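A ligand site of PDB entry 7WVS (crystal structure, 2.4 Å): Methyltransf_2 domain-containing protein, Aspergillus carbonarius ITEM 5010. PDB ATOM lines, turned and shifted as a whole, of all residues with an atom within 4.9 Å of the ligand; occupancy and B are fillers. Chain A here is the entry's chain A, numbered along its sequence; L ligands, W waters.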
ATOM      1  N   GLY A 190      -0.255   1.684 -16.092  1.00  0.00           N
ATOM      2  CA  GLY A 190      -0.567   0.314 -15.686  1.00  0.00           C
ATOM      3  C   GLY A 190      -0.752  -0.624 -16.870  1.00  0.00           C
ATOM      4  O   GLY A 190      -0.259  -1.756 -16.847  1.00  0.00           O
ATOM      5  N   MET A 203       7.660  -5.787 -11.919  1.00  0.00           N
ATOM      6  CA  MET A 203       6.780  -4.913 -11.160  1.00  0.00           C
ATOM      7  C   MET A 203       6.214  -5.628  -9.934  1.00  0.00           C
ATOM      8  O   MET A 203       6.277  -5.126  -8.810  1.00  0.00           O
ATOM      9  CB  MET A 203       5.676  -4.394 -12.074  1.00  0.00           C
ATOM     10  CG  MET A 203       4.793  -3.356 -11.433  1.00  0.00           C
ATOM     11  SD  MET A 203       3.533  -4.081 -10.378  1.00  0.00           S
ATOM     12  CE  MET A 203       2.401  -4.770 -11.594  1.00  0.00           C
ATOM     13  N   MET A 207       6.809  -4.845  -5.551  1.00  0.00           N
ATOM     14  CA  MET A 207       5.824  -4.364  -4.582  1.00  0.00           C
ATOM     15  C   MET A 207       6.072  -4.910  -3.187  1.00  0.00           C
ATOM     16  O   MET A 207       5.491  -4.390  -2.226  1.00  0.00           O
ATOM     17  CB  MET A 207       4.393  -4.685  -5.029  1.00  0.00           C
ATOM     18  CG  MET A 207       3.927  -3.921  -6.260  1.00  0.00           C
ATOM     19  SD  MET A 207       4.019  -2.104  -6.097  1.00  0.00           S
ATOM     20  CE  MET A 207       4.817  -1.655  -7.621  1.00  0.00           C
ATOM     21  N   HIS A 216       3.466  -3.624   4.837  1.00  0.00           N
ATOM     22  CA  HIS A 216       2.257  -4.362   4.513  1.00  0.00           C
ATOM     23  C   HIS A 216       1.407  -4.707   5.729  1.00  0.00           C
ATOM     24  O   HIS A 216       0.213  -4.950   5.595  1.00  0.00           O
ATOM     25  CB  HIS A 216       2.615  -5.628   3.751  1.00  0.00           C
ATOM     26  CG  HIS A 216       3.151  -5.374   2.384  1.00  0.00           C
ATOM     27  ND1 HIS A 216       2.372  -5.449   1.248  1.00  0.00           N
ATOM     28  CD2 HIS A 216       4.401  -5.019   1.969  1.00  0.00           C
ATOM     29  CE1 HIS A 216       3.115  -5.167   0.190  1.00  0.00           C
ATOM     30  NE2 HIS A 216       4.341  -4.897   0.601  1.00  0.00           N
ATOM     31  N   ASP A 240      -9.030  -6.777  -2.844  1.00  0.00           N
ATOM     32  CA  ASP A 240      -7.745  -6.106  -3.013  1.00  0.00           C
ATOM     33  C   ASP A 240      -7.708  -5.461  -4.392  1.00  0.00           C
ATOM     34  O   ASP A 240      -7.391  -6.126  -5.391  1.00  0.00           O
ATOM     35  CB  ASP A 240      -6.612  -7.126  -2.863  1.00  0.00           C
ATOM     36  CG  ASP A 240      -5.267  -6.474  -2.575  1.00  0.00           C
ATOM     37  OD1 ASP A 240      -5.206  -5.222  -2.541  1.00  0.00           O
ATOM     38  OD2 ASP A 240      -4.278  -7.223  -2.373  1.00  0.00           O
ATOM     39  N   ILE A 241      -8.009  -4.170  -4.444  1.00  0.00           N
ATOM     40  CA  ILE A 241      -8.185  -3.462  -5.715  1.00  0.00           C
ATOM     41  C   ILE A 241      -6.813  -3.022  -6.253  1.00  0.00           C
ATOM     42  O   ILE A 241      -6.140  -2.181  -5.649  1.00  0.00           O
ATOM     43  CB  ILE A 241      -9.124  -2.265  -5.543  1.00  0.00           C
ATOM     44  CG1 ILE A 241     -10.432  -2.729  -4.892  1.00  0.00           C
ATOM     45  CG2 ILE A 241      -9.366  -1.544  -6.876  1.00  0.00           C
ATOM     46  CD1 ILE A 241     -11.428  -1.619  -4.656  1.00  0.00           C
ATOM     47  N   GLY A 242      -6.430  -3.566  -7.409  1.00  0.00           N
ATOM     48  CA  GLY A 242      -5.081  -3.394  -7.916  1.00  0.00           C
ATOM     49  C   GLY A 242      -4.035  -4.002  -6.992  1.00  0.00           C
ATOM     50  O   GLY A 242      -3.021  -3.365  -6.674  1.00  0.00           O
ATOM     51  N   GLY A 243      -4.270  -5.239  -6.564  1.00  0.00           N
ATOM     52  CA  GLY A 243      -3.456  -5.900  -5.564  1.00  0.00           C
ATOM     53  C   GLY A 243      -2.166  -6.539  -6.034  1.00  0.00           C
ATOM     54  O   GLY A 243      -1.486  -7.182  -5.225  1.00  0.00           O
ATOM     55  N   ALA A 244      -1.789  -6.387  -7.299  1.00  0.00           N
ATOM     56  CA  ALA A 244      -0.524  -6.918  -7.799  1.00  0.00           C
ATOM     57  C   ALA A 244      -0.578  -8.436  -7.673  1.00  0.00           C
ATOM     58  O   ALA A 244      -1.455  -9.055  -8.306  1.00  0.00           O
ATOM     59  CB  ALA A 244       0.634  -6.220  -7.094  1.00  0.00           C
ATOM     60  N   THR A 248       0.055  -8.355  -0.109  1.00  0.00           N
ATOM     61  CA  THR A 248      -0.642  -7.740   1.019  1.00  0.00           C
ATOM     62  C   THR A 248      -1.768  -8.626   1.550  1.00  0.00           C
ATOM     63  O   THR A 248      -2.035  -8.628   2.759  1.00  0.00           O
ATOM     64  CB  THR A 248      -1.183  -6.355   0.626  1.00  0.00           C
ATOM     65  OG1 THR A 248      -0.169  -5.659  -0.100  1.00  0.00           O
ATOM     66  CG2 THR A 248      -1.541  -5.538   1.858  1.00  0.00           C
ATOM     67  N   ASP A 268      -6.685  -7.102 -10.467  1.00  0.00           N
ATOM     68  CA  ASP A 268      -5.688  -6.311 -11.166  1.00  0.00           C
ATOM     69  C   ASP A 268      -5.992  -6.382 -12.648  1.00  0.00           C
ATOM     70  O   ASP A 268      -7.001  -6.961 -13.066  1.00  0.00           O
ATOM     71  CB  ASP A 268      -4.259  -6.797 -10.835  1.00  0.00           C
ATOM     72  CG  ASP A 268      -3.258  -5.640 -10.811  1.00  0.00           C
ATOM     73  OD1 ASP A 268      -2.978  -5.074 -11.887  1.00  0.00           O
ATOM     74  OD2 ASP A 268      -2.786  -5.274  -9.720  1.00  0.00           O
ATOM     75  N   LEU A 269      -5.128  -5.763 -13.455  1.00  0.00           N
ATOM     76  CA  LEU A 269      -5.306  -5.792 -14.898  1.00  0.00           C
ATOM     77  C   LEU A 269      -5.136  -7.211 -15.423  1.00  0.00           C
ATOM     78  O   LEU A 269      -4.393  -8.024 -14.863  1.00  0.00           O
ATOM     79  CB  LEU A 269      -4.313  -4.863 -15.597  1.00  0.00           C
ATOM     80  CG  LEU A 269      -4.571  -3.346 -15.453  1.00  0.00           C
ATOM     81  CD1 LEU A 269      -3.323  -2.583 -15.815  1.00  0.00           C
ATOM     82  CD2 LEU A 269      -5.753  -2.854 -16.278  1.00  0.00           C
ATOM     83  N   VAL A 272      -1.674  -8.576 -15.640  1.00  0.00           N
ATOM     84  CA  VAL A 272      -1.038  -8.762 -14.337  1.00  0.00           C
ATOM     85  C   VAL A 272      -1.609  -9.973 -13.632  1.00  0.00           C
ATOM     86  O   VAL A 272      -0.878 -10.816 -13.097  1.00  0.00           O
ATOM     87  CB  VAL A 272      -1.212  -7.493 -13.484  1.00  0.00           C
ATOM     88  CG1 VAL A 272      -0.793  -7.745 -12.043  1.00  0.00           C
ATOM     89  CG2 VAL A 272      -0.437  -6.311 -14.118  1.00  0.00           C
ATOM     90  N   ILE A 292      -9.840  -6.826 -13.738  1.00  0.00           N
ATOM     91  CA  ILE A 292     -10.717  -5.662 -13.715  1.00  0.00           C
ATOM     92  C   ILE A 292     -10.015  -4.501 -14.388  1.00  0.00           C
ATOM     93  O   ILE A 292      -8.833  -4.562 -14.722  1.00  0.00           O
ATOM     94  CB  ILE A 292     -11.116  -5.237 -12.277  1.00  0.00           C
ATOM     95  CG1 ILE A 292      -9.941  -4.499 -11.623  1.00  0.00           C
ATOM     96  CG2 ILE A 292     -11.557  -6.415 -11.453  1.00  0.00           C
ATOM     97  CD1 ILE A 292     -10.267  -3.815 -10.307  1.00  0.00           C
ATOM     98  N   ASP A 293     -10.764  -3.417 -14.564  1.00  0.00           N
ATOM     99  CA  ASP A 293     -10.207  -2.107 -14.893  1.00  0.00           C
ATOM    100  C   ASP A 293     -10.822  -1.114 -13.907  1.00  0.00           C
ATOM    101  O   ASP A 293     -11.978  -0.715 -14.067  1.00  0.00           O
ATOM    102  CB  ASP A 293     -10.512  -1.752 -16.336  1.00  0.00           C
ATOM    103  CG  ASP A 293      -9.893  -0.444 -16.753  1.00  0.00           C
ATOM    104  OD1 ASP A 293      -9.340   0.287 -15.878  1.00  0.00           O
ATOM    105  OD2 ASP A 293      -9.950  -0.160 -17.968  1.00  0.00           O
ATOM    106  N   PHE A 294     -10.052  -0.710 -12.883  1.00  0.00           N
ATOM    107  CA  PHE A 294     -10.692   0.115 -11.862  1.00  0.00           C
ATOM    108  C   PHE A 294     -10.984   1.538 -12.324  1.00  0.00           C
ATOM    109  O   PHE A 294     -11.650   2.276 -11.599  1.00  0.00           O
ATOM    110  CB  PHE A 294      -9.885   0.100 -10.539  1.00  0.00           C
ATOM    111  CG  PHE A 294      -8.437   0.553 -10.637  1.00  0.00           C
ATOM    112  CD1 PHE A 294      -8.086   1.755 -11.238  1.00  0.00           C
ATOM    113  CD2 PHE A 294      -7.425  -0.197 -10.027  1.00  0.00           C
ATOM    114  CE1 PHE A 294      -6.752   2.182 -11.283  1.00  0.00           C
ATOM    115  CE2 PHE A 294      -6.083   0.211 -10.052  1.00  0.00           C
ATOM    116  CZ  PHE A 294      -5.736   1.413 -10.683  1.00  0.00           C
ATOM    117  N   HIS A 295     -10.530   1.930 -13.525  1.00  0.00           N
ATOM    118  CA  HIS A 295     -10.977   3.216 -14.093  1.00  0.00           C
ATOM    119  C   HIS A 295     -12.436   3.174 -14.527  1.00  0.00           C
ATOM    120  O   HIS A 295     -13.055   4.230 -14.703  1.00  0.00           O
ATOM    121  CB  HIS A 295     -10.115   3.596 -15.301  1.00  0.00           C
ATOM    122  CG  HIS A 295      -8.676   3.841 -14.971  1.00  0.00           C
ATOM    123  ND1 HIS A 295      -8.287   4.740 -14.002  1.00  0.00           N
ATOM    124  CD2 HIS A 295      -7.546   3.303 -15.473  1.00  0.00           C
ATOM    125  CE1 HIS A 295      -6.964   4.743 -13.925  1.00  0.00           C
ATOM    126  NE2 HIS A 295      -6.493   3.878 -14.802  1.00  0.00           N
ATOM    127  N   ARG A 309      -4.712  -0.018  -2.010  1.00  0.00           N
ATOM    128  CA  ARG A 309      -3.372   0.120  -1.455  1.00  0.00           C
ATOM    129  C   ARG A 309      -2.413   0.603  -2.535  1.00  0.00           C
ATOM    130  O   ARG A 309      -2.227  -0.089  -3.546  1.00  0.00           O
ATOM    131  CB  ARG A 309      -2.861  -1.189  -0.845  1.00  0.00           C
ATOM    132  CG  ARG A 309      -1.393  -1.076  -0.336  1.00  0.00           C
ATOM    133  CD  ARG A 309      -0.767  -2.417   0.085  1.00  0.00           C
ATOM    134  NE  ARG A 309       0.703  -2.344   0.106  1.00  0.00           N
ATOM    135  CZ  ARG A 309       1.432  -2.007   1.174  1.00  0.00           C
ATOM    136  NH1 ARG A 309       0.830  -1.755   2.337  1.00  0.00           N
ATOM    137  NH2 ARG A 309       2.763  -1.938   1.076  1.00  0.00           N
ATOM    138  N   ARG A 310      -1.797   1.755  -2.295  1.00  0.00           N
ATOM    139  CA  ARG A 310      -0.807   2.332  -3.206  1.00  0.00           C
ATOM    140  C   ARG A 310      -1.372   2.375  -4.623  1.00  0.00           C
ATOM    141  O   ARG A 310      -0.742   1.973  -5.593  1.00  0.00           O
ATOM    142  CB  ARG A 310       0.502   1.554  -3.133  1.00  0.00           C
ATOM    143  CG  ARG A 310       0.953   1.356  -1.674  1.00  0.00           C
ATOM    144  CD  ARG A 310       2.338   0.738  -1.572  1.00  0.00           C
ATOM    145  NE  ARG A 310       3.318   1.625  -2.174  1.00  0.00           N
ATOM    146  CZ  ARG A 310       4.376   1.213  -2.862  1.00  0.00           C
ATOM    147  NH1 ARG A 310       4.605  -0.086  -3.042  1.00  0.00           N
ATOM    148  NH2 ARG A 310       5.204   2.114  -3.367  1.00  0.00           N
ATOM    149  N   ILE A 311      -2.614   2.853  -4.713  1.00  0.00           N
ATOM    150  CA  ILE A 311      -3.283   3.060  -5.982  1.00  0.00           C
ATOM    151  C   ILE A 311      -3.425   4.541  -6.277  1.00  0.00           C
ATOM    152  O   ILE A 311      -2.985   5.021  -7.317  1.00  0.00           O
ATOM    153  CB  ILE A 311      -4.653   2.350  -5.999  1.00  0.00           C
ATOM    154  CG1 ILE A 311      -4.462   0.848  -5.744  1.00  0.00           C
ATOM    155  CG2 ILE A 311      -5.350   2.642  -7.297  1.00  0.00           C
ATOM    156  CD1 ILE A 311      -3.602   0.120  -6.743  1.00  0.00           C
ATOM    157  N   ARG A 313      -1.905   7.078  -5.368  1.00  0.00           N
ATOM    158  CA  ARG A 313      -0.636   7.732  -5.659  1.00  0.00           C
ATOM    159  C   ARG A 313      -0.364   7.804  -7.160  1.00  0.00           C
ATOM    160  O   ARG A 313       0.346   8.702  -7.619  1.00  0.00           O
ATOM    161  CB  ARG A 313       0.523   6.995  -4.975  1.00  0.00           C
ATOM    162  CG  ARG A 313       0.696   5.555  -5.439  1.00  0.00           C
ATOM    163  CD  ARG A 313       1.552   4.742  -4.478  1.00  0.00           C
ATOM    164  NE  ARG A 313       2.964   5.098  -4.561  1.00  0.00           N
ATOM    165  CZ  ARG A 313       3.562   5.986  -3.770  1.00  0.00           C
ATOM    166  NH1 ARG A 313       2.862   6.587  -2.816  1.00  0.00           N
ATOM    167  NH2 ARG A 313       4.840   6.280  -3.938  1.00  0.00           N
ATOM    168  N   ASP A 314      -0.909   6.862  -7.933  1.00  0.00           N
ATOM    169  CA  ASP A 314      -0.588   6.743  -9.352  1.00  0.00           C
ATOM    170  C   ASP A 314      -1.428   7.643 -10.247  1.00  0.00           C
ATOM    171  O   ASP A 314      -1.247   7.610 -11.464  1.00  0.00           O
ATOM    172  CB  ASP A 314      -0.754   5.279  -9.811  1.00  0.00           C
ATOM    173  CG  ASP A 314       0.423   4.398  -9.394  1.00  0.00           C
ATOM    174  OD1 ASP A 314       1.390   4.921  -8.787  1.00  0.00           O
ATOM    175  OD2 ASP A 314       0.358   3.172  -9.648  1.00  0.00           O
ATOM    176  N   PHE A 315      -2.343   8.440  -9.700  1.00  0.00           N
ATOM    177  CA  PHE A 315      -3.244   9.221 -10.551  1.00  0.00           C
ATOM    178  C   PHE A 315      -3.499  10.584  -9.932  1.00  0.00           C
ATOM    179  O   PHE A 315      -3.309  10.803  -8.732  1.00  0.00           O
ATOM    180  CB  PHE A 315      -4.571   8.469 -10.777  1.00  0.00           C
ATOM    181  CG  PHE A 315      -4.373   7.068 -11.286  1.00  0.00           C
ATOM    182  CD1 PHE A 315      -4.216   6.836 -12.653  1.00  0.00           C
ATOM    183  CD2 PHE A 315      -4.268   6.007 -10.393  1.00  0.00           C
ATOM    184  CE1 PHE A 315      -3.998   5.561 -13.111  1.00  0.00           C
ATOM    185  CE2 PHE A 315      -4.050   4.732 -10.851  1.00  0.00           C
ATOM    186  CZ  PHE A 315      -3.917   4.500 -12.218  1.00  0.00           C
HETATM  187  N1  LIG L   1      -1.587  -2.903  -4.371  1.00  0.00           N
HETATM  188  C1  LIG L   1      -0.254  -3.399  -4.662  1.00  0.00           C
HETATM  189  C2  LIG L   1       0.716  -3.005  -3.557  1.00  0.00           C
HETATM  190  O1  LIG L   1       0.523  -2.010  -2.876  1.00  0.00           O
HETATM  191  O2  LIG L   1       1.721  -3.670  -3.343  1.00  0.00           O
HETATM  192  C3  LIG L   1       0.241  -2.877  -6.001  1.00  0.00           C
HETATM  193  C4  LIG L   1       0.367  -1.349  -6.036  1.00  0.00           C
HETATM  194  S1  LIG L   1       1.058  -0.789  -7.613  1.00  0.00           S
HETATM  195  C5  LIG L   1       1.713   0.843  -7.116  1.00  0.00           C
HETATM  196  C6  LIG L   1      -0.421  -0.349  -8.569  1.00  0.00           C
HETATM  197  C7  LIG L   1      -1.171  -1.588  -9.041  1.00  0.00           C
HETATM  198  O3  LIG L   1      -2.357  -1.209  -9.708  1.00  0.00           O
HETATM  199  C8  LIG L   1      -0.376  -2.418 -10.039  1.00  0.00           C
HETATM  200  O4  LIG L   1      -0.488  -3.775  -9.653  1.00  0.00           O
HETATM  201  C9  LIG L   1      -1.069  -2.183 -11.373  1.00  0.00           C
HETATM  202  O5  LIG L   1      -0.972  -3.276 -12.270  1.00  0.00           O
HETATM  203  C10 LIG L   1      -2.496  -1.965 -10.900  1.00  0.00           C
HETATM  204  N2  LIG L   1      -3.331  -1.233 -11.855  1.00  0.00           N
HETATM  205  C11 LIG L   1      -2.984  -0.100 -12.571  1.00  0.00           C
HETATM  206  N3  LIG L   1      -4.052   0.275 -13.321  1.00  0.00           N
HETATM  207  C12 LIG L   1      -5.071  -0.591 -13.081  1.00  0.00           C
HETATM  208  C13 LIG L   1      -6.367  -0.676 -13.583  1.00  0.00           C
HETATM  209  N4  LIG L   1      -6.815   0.211 -14.479  1.00  0.00           N
HETATM  210  N5  LIG L   1      -7.191  -1.699 -13.146  1.00  0.00           N
HETATM  211  C14 LIG L   1      -6.722  -2.625 -12.234  1.00  0.00           C
HETATM  212  N6  LIG L   1      -5.435  -2.540 -11.738  1.00  0.00           N
HETATM  213  C15 LIG L   1      -4.627  -1.549 -12.158  1.00  0.00           C
HETATM  214  O   HOH W   1      -2.461  -4.689  -2.315  1.00  0.00           O
HETATM  215  O   HOH W   2      -4.888  -2.450  -3.346  1.00  0.00           O
HETATM  216  O   HOH W   3       3.671  -2.454  -1.708  1.00  0.00           O
HETATM  217  O   HOH W   4       1.183  -6.209  -2.754  1.00  0.00           O
HETATM  218  O   HOH W   5       0.754  -2.771 -14.411  1.00  0.00           O
HETATM  219  O   HOH W   6      -4.116   2.435 -15.081  1.00  0.00           O
HETATM  220  O   HOH W   7      -0.563   2.083 -12.220  1.00  0.00           O
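A nitrogen (N1) of the ligand sits at hydrogen-bond distance from the backbone carbonyl oxygen of Gly 242, 2.8 Å away. N of Phe 294 sits at hydrogen-bond distance from N5 of the ligand, 3.0 Å away. N4 of the ligand is in hydrogen-bond range of OD1 of Asp 293 (2.9 Å). The guanidinium group of Arg 309 is in salt-bridge range of an oxygen (O1) of the ligand, 3.0 Å away. The side-chain carboxylate of Asp 268 lies within hydrogen-bond range of an oxygen (O5) of the ligand (2.7 Å). The backbone carbonyl oxygen of Arg 309 is in hydrogen-bond range of a nitrogen (N1) of the ligand, at 3.0 Å.
The backbone carbonyl oxygen (O) of Asp 268 is in hydrogen-bond range of the backbone NH (N) of Ile 292, 2.9 Å away. NH1 of Arg 310 lies within hydrogen-bond range of SD of Met 207, 3.7 Å away. NE of Arg 309 sits close to OG1 of Thr 248, at 3.4 Å. NE2 of His 216 sits at hydrogen-bond distance from O of Met 207 (3.1 Å). OD2 of Asp 268 is in hydrogen-bond range of N of Gly 243 (3.5 Å). The backbone NH (N) of His 295 sits close to the side-chain carboxylate (OD1) of Asp 293, at 3.1 Å. NH2 of Arg 309 lies close to NE2 of His 216 (3.4 Å). The backbone NH of Ala 244 is in hydrogen-bond range of the side-chain carboxylate of Asp 268.
The side-chain sulfur (SD) of Met 207 lies close to a sulfur (S1) of the ligand, at 3.6 Å. Gly 190 touches the ligand. Met 203 touches the ligand. CA of Gly 243 touches N1 of the ligand, at 3.7 Å. Ala 244 touches the ligand. Leu 269 touches the ligand (CD2 to C13, 3.5 Å). Val 272 touches the ligand (CG2 to O5, 3.6 Å). Ile 292 touches the ligand. His 295 touches the ligand. Arg 310 touches the ligand. Ile 311 touches the ligand (CD1 to O3, 3.5 Å). Asp 314 touches the ligand (OD2 to C5, 3.7 Å). Hydrophobic or aromatic side chains that line the ligand: Met 203, Met 207, Ala 244, Leu 269, Val 272, Ile 292, Phe 294, His 295 and Ile 311.
Water W4 lies within hydrogen-bond range of O2 of the ligand (2.7 Å) and OG1 of Thr 248 (3.0 Å). Water W6 lies within hydrogen-bond range of N3 of the ligand and NE2 of His 295. Water W5 bridges an oxygen (O5) of the ligand and the backbone carbonyl oxygen (O) of Gly 190. Water W3 lies within hydrogen-bond range of the backbone carbonyl oxygen (O) of Met 207 (2.7 Å), an oxygen (O2) of the ligand (2.8 Å), the guanidinium group (NH1) of Arg 310 (2.9 Å), the guanidinium group (NH2) of Arg 309 (3.0 Å) and a ring nitrogen (NE2) of His 216 (3.4 Å). Water W1 lies within hydrogen-bond range of the side-chain carboxylate (OD1) of Asp 240 (2.8 Å), a nitrogen (N1) of the ligand (2.9 Å) and the side-chain hydroxyl (OG1) of Thr 248 (3.3 Å). Water W2 lies within hydrogen-bond range of O of Ile 241 (2.6 Å), N of Arg 309 (2.8 Å), OD1 of Asp 240 (2.9 Å) and N1 of the ligand (3.5 Å).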
